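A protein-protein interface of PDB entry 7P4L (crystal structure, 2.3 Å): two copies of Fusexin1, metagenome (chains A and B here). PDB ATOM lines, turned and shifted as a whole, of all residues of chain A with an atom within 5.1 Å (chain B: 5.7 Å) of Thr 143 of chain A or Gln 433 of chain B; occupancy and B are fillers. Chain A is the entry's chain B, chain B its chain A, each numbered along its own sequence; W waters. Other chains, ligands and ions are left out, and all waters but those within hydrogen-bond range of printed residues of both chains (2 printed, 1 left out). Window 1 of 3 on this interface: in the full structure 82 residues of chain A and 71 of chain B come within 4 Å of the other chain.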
ATOM      1  N   THR A  72     -25.330  -4.988  -3.862  1.00  0.00           N
ATOM      2  CA  THR A  72     -24.141  -5.335  -4.633  1.00  0.00           C
ATOM      3  C   THR A  72     -23.336  -6.419  -3.919  1.00  0.00           C
ATOM      4  O   THR A  72     -23.610  -6.781  -2.773  1.00  0.00           O
ATOM      5  CB  THR A  72     -23.244  -4.120  -4.857  1.00  0.00           C
ATOM      6  OG1 THR A  72     -22.793  -3.621  -3.592  1.00  0.00           O
ATOM      7  CG2 THR A  72     -23.973  -3.022  -5.616  1.00  0.00           C
ATOM      8  N   ASP A  78     -18.602  -6.605 -12.538  1.00  0.00           N
ATOM      9  CA  ASP A  78     -19.093  -5.675 -13.542  1.00  0.00           C
ATOM     10  C   ASP A  78     -19.261  -6.368 -14.886  1.00  0.00           C
ATOM     11  O   ASP A  78     -18.591  -7.359 -15.197  1.00  0.00           O
ATOM     12  CB  ASP A  78     -18.131  -4.496 -13.704  1.00  0.00           C
ATOM     13  CG  ASP A  78     -18.015  -3.649 -12.448  1.00  0.00           C
ATOM     14  OD1 ASP A  78     -18.940  -3.688 -11.609  1.00  0.00           O
ATOM     15  OD2 ASP A  78     -17.008  -2.922 -12.315  1.00  0.00           O
ATOM     16  N   LYS A 140     -17.137  -0.407 -19.362  1.00  0.00           N
ATOM     17  CA  LYS A 140     -17.994  -1.007 -18.350  1.00  0.00           C
ATOM     18  C   LYS A 140     -19.433  -0.733 -18.757  1.00  0.00           C
ATOM     19  O   LYS A 140     -19.844   0.429 -18.837  1.00  0.00           O
ATOM     20  CB  LYS A 140     -17.712  -0.437 -16.962  1.00  0.00           C
ATOM     21  CG  LYS A 140     -18.545  -1.080 -15.862  1.00  0.00           C
ATOM     22  CD  LYS A 140     -18.767  -0.142 -14.676  1.00  0.00           C
ATOM     23  CE  LYS A 140     -17.500   0.094 -13.892  1.00  0.00           C
ATOM     24  NZ  LYS A 140     -17.754   0.912 -12.675  1.00  0.00           N
ATOM     25  N   LEU A 141     -20.193  -1.793 -19.032  1.00  0.00           N
ATOM     26  CA  LEU A 141     -21.569  -1.601 -19.474  1.00  0.00           C
ATOM     27  C   LEU A 141     -22.515  -1.362 -18.302  1.00  0.00           C
ATOM     28  O   LEU A 141     -23.462  -0.578 -18.427  1.00  0.00           O
ATOM     29  CB  LEU A 141     -22.030  -2.800 -20.300  1.00  0.00           C
ATOM     30  CG  LEU A 141     -21.263  -3.039 -21.599  1.00  0.00           C
ATOM     31  CD1 LEU A 141     -21.851  -4.234 -22.326  1.00  0.00           C
ATOM     32  CD2 LEU A 141     -21.311  -1.796 -22.467  1.00  0.00           C
ATOM     33  N   ALA A 142     -22.284  -2.020 -17.169  1.00  0.00           N
ATOM     34  CA  ALA A 142     -23.141  -1.835 -16.003  1.00  0.00           C
ATOM     35  C   ALA A 142     -22.493  -2.466 -14.783  1.00  0.00           C
ATOM     36  O   ALA A 142     -21.708  -3.411 -14.901  1.00  0.00           O
ATOM     37  CB  ALA A 142     -24.527  -2.454 -16.226  1.00  0.00           C
ATOM     38  N   THR A 143     -22.852  -1.939 -13.607  1.00  0.00           N
ATOM     39  CA  THR A 143     -22.541  -2.567 -12.331  1.00  0.00           C
ATOM     40  C   THR A 143     -23.774  -3.318 -11.855  1.00  0.00           C
ATOM     41  O   THR A 143     -24.811  -2.682 -11.610  1.00  0.00           O
ATOM     42  CB  THR A 143     -22.128  -1.525 -11.294  1.00  0.00           C
ATOM     43  OG1 THR A 143     -20.951  -0.831 -11.734  1.00  0.00           O
ATOM     44  CG2 THR A 143     -21.855  -2.178  -9.947  1.00  0.00           C
ATOM     45  N   PRO A 144     -23.734  -4.641 -11.736  1.00  0.00           N
ATOM     46  CA  PRO A 144     -24.938  -5.387 -11.361  1.00  0.00           C
ATOM     47  C   PRO A 144     -25.183  -5.399  -9.857  1.00  0.00           C
ATOM     48  O   PRO A 144     -24.276  -5.212  -9.042  1.00  0.00           O
ATOM     49  CB  PRO A 144     -24.634  -6.799 -11.875  1.00  0.00           C
ATOM     50  CG  PRO A 144     -23.159  -6.914 -11.736  1.00  0.00           C
ATOM     51  CD  PRO A 144     -22.596  -5.542 -11.997  1.00  0.00           C
ATOM     52  N   ALA A 145     -26.440  -5.660  -9.500  1.00  0.00           N
ATOM     53  CA  ALA A 145     -26.837  -5.785  -8.105  1.00  0.00           C
ATOM     54  C   ALA A 145     -28.043  -6.704  -8.006  1.00  0.00           C
ATOM     55  O   ALA A 145     -28.908  -6.716  -8.885  1.00  0.00           O
ATOM     56  CB  ALA A 145     -27.181  -4.431  -7.484  1.00  0.00           C
ATOM     57  N   ALA A 210     -30.531  -5.941 -10.997  1.00  0.00           N
ATOM     58  CA  ALA A 210     -30.435  -4.520 -11.298  1.00  0.00           C
ATOM     59  C   ALA A 210     -29.121  -4.250 -12.011  1.00  0.00           C
ATOM     60  O   ALA A 210     -28.104  -4.880 -11.712  1.00  0.00           O
ATOM     61  CB  ALA A 210     -30.520  -3.677 -10.028  1.00  0.00           C
ATOM     62  N   LEU A 211     -29.154  -3.331 -12.974  1.00  0.00           N
ATOM     63  CA  LEU A 211     -27.984  -2.971 -13.769  1.00  0.00           C
ATOM     64  C   LEU A 211     -27.806  -1.463 -13.679  1.00  0.00           C
ATOM     65  O   LEU A 211     -28.592  -0.708 -14.260  1.00  0.00           O
ATOM     66  CB  LEU A 211     -28.151  -3.404 -15.224  1.00  0.00           C
ATOM     67  CG  LEU A 211     -28.510  -4.863 -15.476  1.00  0.00           C
ATOM     68  CD1 LEU A 211     -28.947  -5.038 -16.920  1.00  0.00           C
ATOM     69  CD2 LEU A 211     -27.354  -5.784 -15.144  1.00  0.00           C
ATOM     70  N   TYR A 212     -26.757  -1.024 -12.991  1.00  0.00           N
ATOM     71  CA  TYR A 212     -26.542   0.398 -12.741  1.00  0.00           C
ATOM     72  C   TYR A 212     -25.623   0.992 -13.804  1.00  0.00           C
ATOM     73  O   TYR A 212     -24.514   0.493 -14.025  1.00  0.00           O
ATOM     74  CB  TYR A 212     -25.953   0.604 -11.348  1.00  0.00           C
ATOM     75  CG  TYR A 212     -26.978   0.541 -10.230  1.00  0.00           C
ATOM     76  CD1 TYR A 212     -27.319  -0.668  -9.635  1.00  0.00           C
ATOM     77  CD2 TYR A 212     -27.596   1.694  -9.765  1.00  0.00           C
ATOM     78  CE1 TYR A 212     -28.247  -0.727  -8.618  1.00  0.00           C
ATOM     79  CE2 TYR A 212     -28.528   1.645  -8.745  1.00  0.00           C
ATOM     80  CZ  TYR A 212     -28.845   0.434  -8.174  1.00  0.00           C
ATOM     81  OH  TYR A 212     -29.770   0.386  -7.160  1.00  0.00           O
ATOM     82  N   LYS B 340     -24.201   4.424  -0.896  1.00  0.00           N
ATOM     83  CA  LYS B 340     -23.504   4.108  -2.134  1.00  0.00           C
ATOM     84  C   LYS B 340     -24.511   3.554  -3.134  1.00  0.00           C
ATOM     85  O   LYS B 340     -25.186   2.556  -2.855  1.00  0.00           O
ATOM     86  CB  LYS B 340     -22.376   3.106  -1.880  1.00  0.00           C
ATOM     87  CG  LYS B 340     -21.679   2.600  -3.141  1.00  0.00           C
ATOM     88  CD  LYS B 340     -21.137   3.747  -3.986  1.00  0.00           C
ATOM     89  CE  LYS B 340     -20.271   3.245  -5.132  1.00  0.00           C
ATOM     90  NZ  LYS B 340     -19.011   2.610  -4.657  1.00  0.00           N
ATOM     91  N   GLU B 341     -24.621   4.217  -4.282  1.00  0.00           N
ATOM     92  CA  GLU B 341     -25.466   3.755  -5.372  1.00  0.00           C
ATOM     93  C   GLU B 341     -25.296   2.255  -5.562  1.00  0.00           C
ATOM     94  O   GLU B 341     -24.178   1.766  -5.734  1.00  0.00           O
ATOM     95  CB  GLU B 341     -25.084   4.513  -6.652  1.00  0.00           C
ATOM     96  CG  GLU B 341     -26.151   4.581  -7.737  1.00  0.00           C
ATOM     97  CD  GLU B 341     -25.744   5.487  -8.911  1.00  0.00           C
ATOM     98  OE1 GLU B 341     -24.544   5.554  -9.256  1.00  0.00           O
ATOM     99  OE2 GLU B 341     -26.629   6.129  -9.506  1.00  0.00           O
ATOM    100  N   GLY B 342     -26.404   1.515  -5.476  1.00  0.00           N
ATOM    101  CA  GLY B 342     -26.406   0.068  -5.563  1.00  0.00           C
ATOM    102  C   GLY B 342     -26.595  -0.650  -4.238  1.00  0.00           C
ATOM    103  O   GLY B 342     -26.923  -1.844  -4.238  1.00  0.00           O
ATOM    104  N   ILE B 431     -23.230   8.550  -3.074  1.00  0.00           N
ATOM    105  CA  ILE B 431     -22.016   8.310  -3.847  1.00  0.00           C
ATOM    106  C   ILE B 431     -22.411   7.478  -5.060  1.00  0.00           C
ATOM    107  O   ILE B 431     -22.996   6.399  -4.912  1.00  0.00           O
ATOM    108  CB  ILE B 431     -20.943   7.583  -3.018  1.00  0.00           C
ATOM    109  CG1 ILE B 431     -20.653   8.328  -1.706  1.00  0.00           C
ATOM    110  CG2 ILE B 431     -19.662   7.441  -3.817  1.00  0.00           C
ATOM    111  CD1 ILE B 431     -20.000   9.671  -1.881  1.00  0.00           C
ATOM    112  N   GLN B 432     -22.107   7.977  -6.254  1.00  0.00           N
ATOM    113  CA  GLN B 432     -22.428   7.239  -7.465  1.00  0.00           C
ATOM    114  C   GLN B 432     -21.444   6.095  -7.684  1.00  0.00           C
ATOM    115  O   GLN B 432     -20.289   6.140  -7.246  1.00  0.00           O
ATOM    116  CB  GLN B 432     -22.401   8.148  -8.691  1.00  0.00           C
ATOM    117  CG  GLN B 432     -23.471   9.212  -8.731  1.00  0.00           C
ATOM    118  CD  GLN B 432     -23.767   9.662 -10.153  1.00  0.00           C
ATOM    119  OE1 GLN B 432     -24.370   8.927 -10.931  1.00  0.00           O
ATOM    120  NE2 GLN B 432     -23.331  10.867 -10.501  1.00  0.00           N
ATOM    121  N   GLN B 433     -21.913   5.056  -8.369  1.00  0.00           N
ATOM    122  CA  GLN B 433     -20.987   4.124  -8.996  1.00  0.00           C
ATOM    123  C   GLN B 433     -20.223   4.855 -10.083  1.00  0.00           C
ATOM    124  O   GLN B 433     -20.795   5.650 -10.834  1.00  0.00           O
ATOM    125  CB  GLN B 433     -21.725   2.931  -9.600  1.00  0.00           C
ATOM    126  CG  GLN B 433     -22.394   1.993  -8.596  1.00  0.00           C
ATOM    127  CD  GLN B 433     -21.405   1.056  -7.929  1.00  0.00           C
ATOM    128  OE1 GLN B 433     -20.298   0.851  -8.424  1.00  0.00           O
ATOM    129  NE2 GLN B 433     -21.811   0.462  -6.814  1.00  0.00           N
ATOM    130  N   SER B 434     -18.928   4.577 -10.183  1.00  0.00           N
ATOM    131  CA  SER B 434     -18.156   5.145 -11.276  1.00  0.00           C
ATOM    132  C   SER B 434     -18.574   4.491 -12.584  1.00  0.00           C
ATOM    133  O   SER B 434     -18.881   3.298 -12.631  1.00  0.00           O
ATOM    134  CB  SER B 434     -16.659   4.950 -11.041  1.00  0.00           C
ATOM    135  OG  SER B 434     -16.316   3.575 -11.027  1.00  0.00           O
ATOM    136  N   GLU B 435     -18.610   5.290 -13.650  1.00  0.00           N
ATOM    137  CA  GLU B 435     -18.853   4.750 -14.979  1.00  0.00           C
ATOM    138  C   GLU B 435     -17.586   4.198 -15.617  1.00  0.00           C
ATOM    139  O   GLU B 435     -17.677   3.348 -16.508  1.00  0.00           O
ATOM    140  CB  GLU B 435     -19.448   5.824 -15.895  1.00  0.00           C
ATOM    141  CG  GLU B 435     -20.798   6.349 -15.458  1.00  0.00           C
ATOM    142  CD  GLU B 435     -21.880   5.289 -15.485  1.00  0.00           C
ATOM    143  OE1 GLU B 435     -21.909   4.474 -16.432  1.00  0.00           O
ATOM    144  OE2 GLU B 435     -22.713   5.275 -14.555  1.00  0.00           O
ATOM    145  N   GLY B 460     -14.437   9.983 -12.989  1.00  0.00           N
ATOM    146  CA  GLY B 460     -14.869   8.617 -13.181  1.00  0.00           C
ATOM    147  C   GLY B 460     -16.288   8.488 -13.674  1.00  0.00           C
ATOM    148  O   GLY B 460     -16.898   7.427 -13.514  1.00  0.00           O
ATOM    149  N   LEU B 461     -16.827   9.538 -14.294  1.00  0.00           N
ATOM    150  CA  LEU B 461     -18.201   9.545 -14.765  1.00  0.00           C
ATOM    151  C   LEU B 461     -18.330   9.744 -16.265  1.00  0.00           C
ATOM    152  O   LEU B 461     -19.360   9.365 -16.830  1.00  0.00           O
ATOM    153  CB  LEU B 461     -19.005  10.653 -14.060  1.00  0.00           C
ATOM    154  CG  LEU B 461     -19.120  10.582 -12.530  1.00  0.00           C
ATOM    155  CD1 LEU B 461     -19.798  11.823 -11.979  1.00  0.00           C
ATOM    156  CD2 LEU B 461     -19.873   9.344 -12.089  1.00  0.00           C
HETATM  157  O   HOH W   1     -14.715   1.777 -12.853  1.00  0.00           O
HETATM  158  O   HOH W   2     -29.105   2.578  -5.203  1.00  0.00           O
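Asp 78 of chain A touches none of the printed residues of chain B.
Of the printed residues of chain B, Lys 140 of chain A touches Ser 434 (2.6 Å) and Glu 435 (3.8 Å).
Leu 141 of chain A touches none of the printed residues of chain B.
Thr 143 of chain A touches just one residue of chain B: Gln 433.
Of the printed residues of chain A, Glu 341 of chain B touches Tyr 212.
Of the printed residues of chain A, Gly 342 of chain B touches Thr 72 and Tyr 212.
Gln 433 of chain B touches one residue of chain A.
Printed residues of chain A within 4 Å of Glu 435 of chain B: Lys 140.
The nearest residue of chain B that does not touch Thr 143 of chain A is Ser 434 of chain B (4.7 Å).
The nearest residue of chain A that does not touch Gln 433 of chain B is Thr 72 of chain A (4.3 Å).
NE2 of Gln 433 of chain B is in hydrogen-bond range of O of Glu 341 of chain B.
The backbone NH (N) of Glu 435 of chain B is in hydrogen-bond range of the backbone carbonyl oxygen (O) of Gly 460 of chain B, at 2.7 Å.
The backbone NH (N) of Glu 341 of chain B lies within hydrogen-bond range of the backbone carbonyl oxygen (O) of Ile 431 of chain B.
The side-chain carboxylate (OD1) of Asp 78 of chain A is in hydrogen-bond range of the side-chain hydroxyl (OG1) of Thr 143 of chain A (3.5 Å).
OD2 of Asp 78 of chain A is in salt-bridge range of NZ of Lys 140 of chain A, 3.9 Å away.
The backbone NH of Tyr 212 of chain A sits at hydrogen-bond distance from the backbone carbonyl oxygen of Thr 143 of chain A, at 2.9 Å.
Hydrophobic or aromatic side chains of chain A that line the printed part of chain B: Tyr 212.
Along chain A the printed residues that touch a printed residue of chain B span positions 72 to 212.
Of the 10 printed residues of chain B, 5 touch a printed residue of chain A.
Among the printed residues, no Asp or Glu carboxylate lies within 4 Å of a Lys or Arg side-chain nitrogen of the other chain.
Water W2 bridges the backbone NH of Gly 342 of chain B (2.9 Å) and the side-chain hydroxyl of Tyr 212 of chain A (3.0 Å).
Water W1 bridges OG of Ser 434 of chain B (3.0 Å) and NZ of Lys 140 of chain A (3.2 Å).
The backbone carbonyl oxygen (O) of Ser 434 of chain B lies within hydrogen-bond range of the side-chain amino group (NZ) of Lys 140 of chain A (2.6 Å).
Gly 342 of chain B touches Thr 72 of chain A.
Lys 140 of chain A touches Glu 435 of chain B.
Gln 433 of chain B touches Thr 143 of chain A (OE1 to CG2, 3.7 Å).
CD2 of Tyr 212 of chain A touches CG of Glu 341 of chain B, 3.8 Å away.
Gly 342 of chain B touches Tyr 212 of chain A (CA to CZ, 3.6 Å).
No position is printed for both chains.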
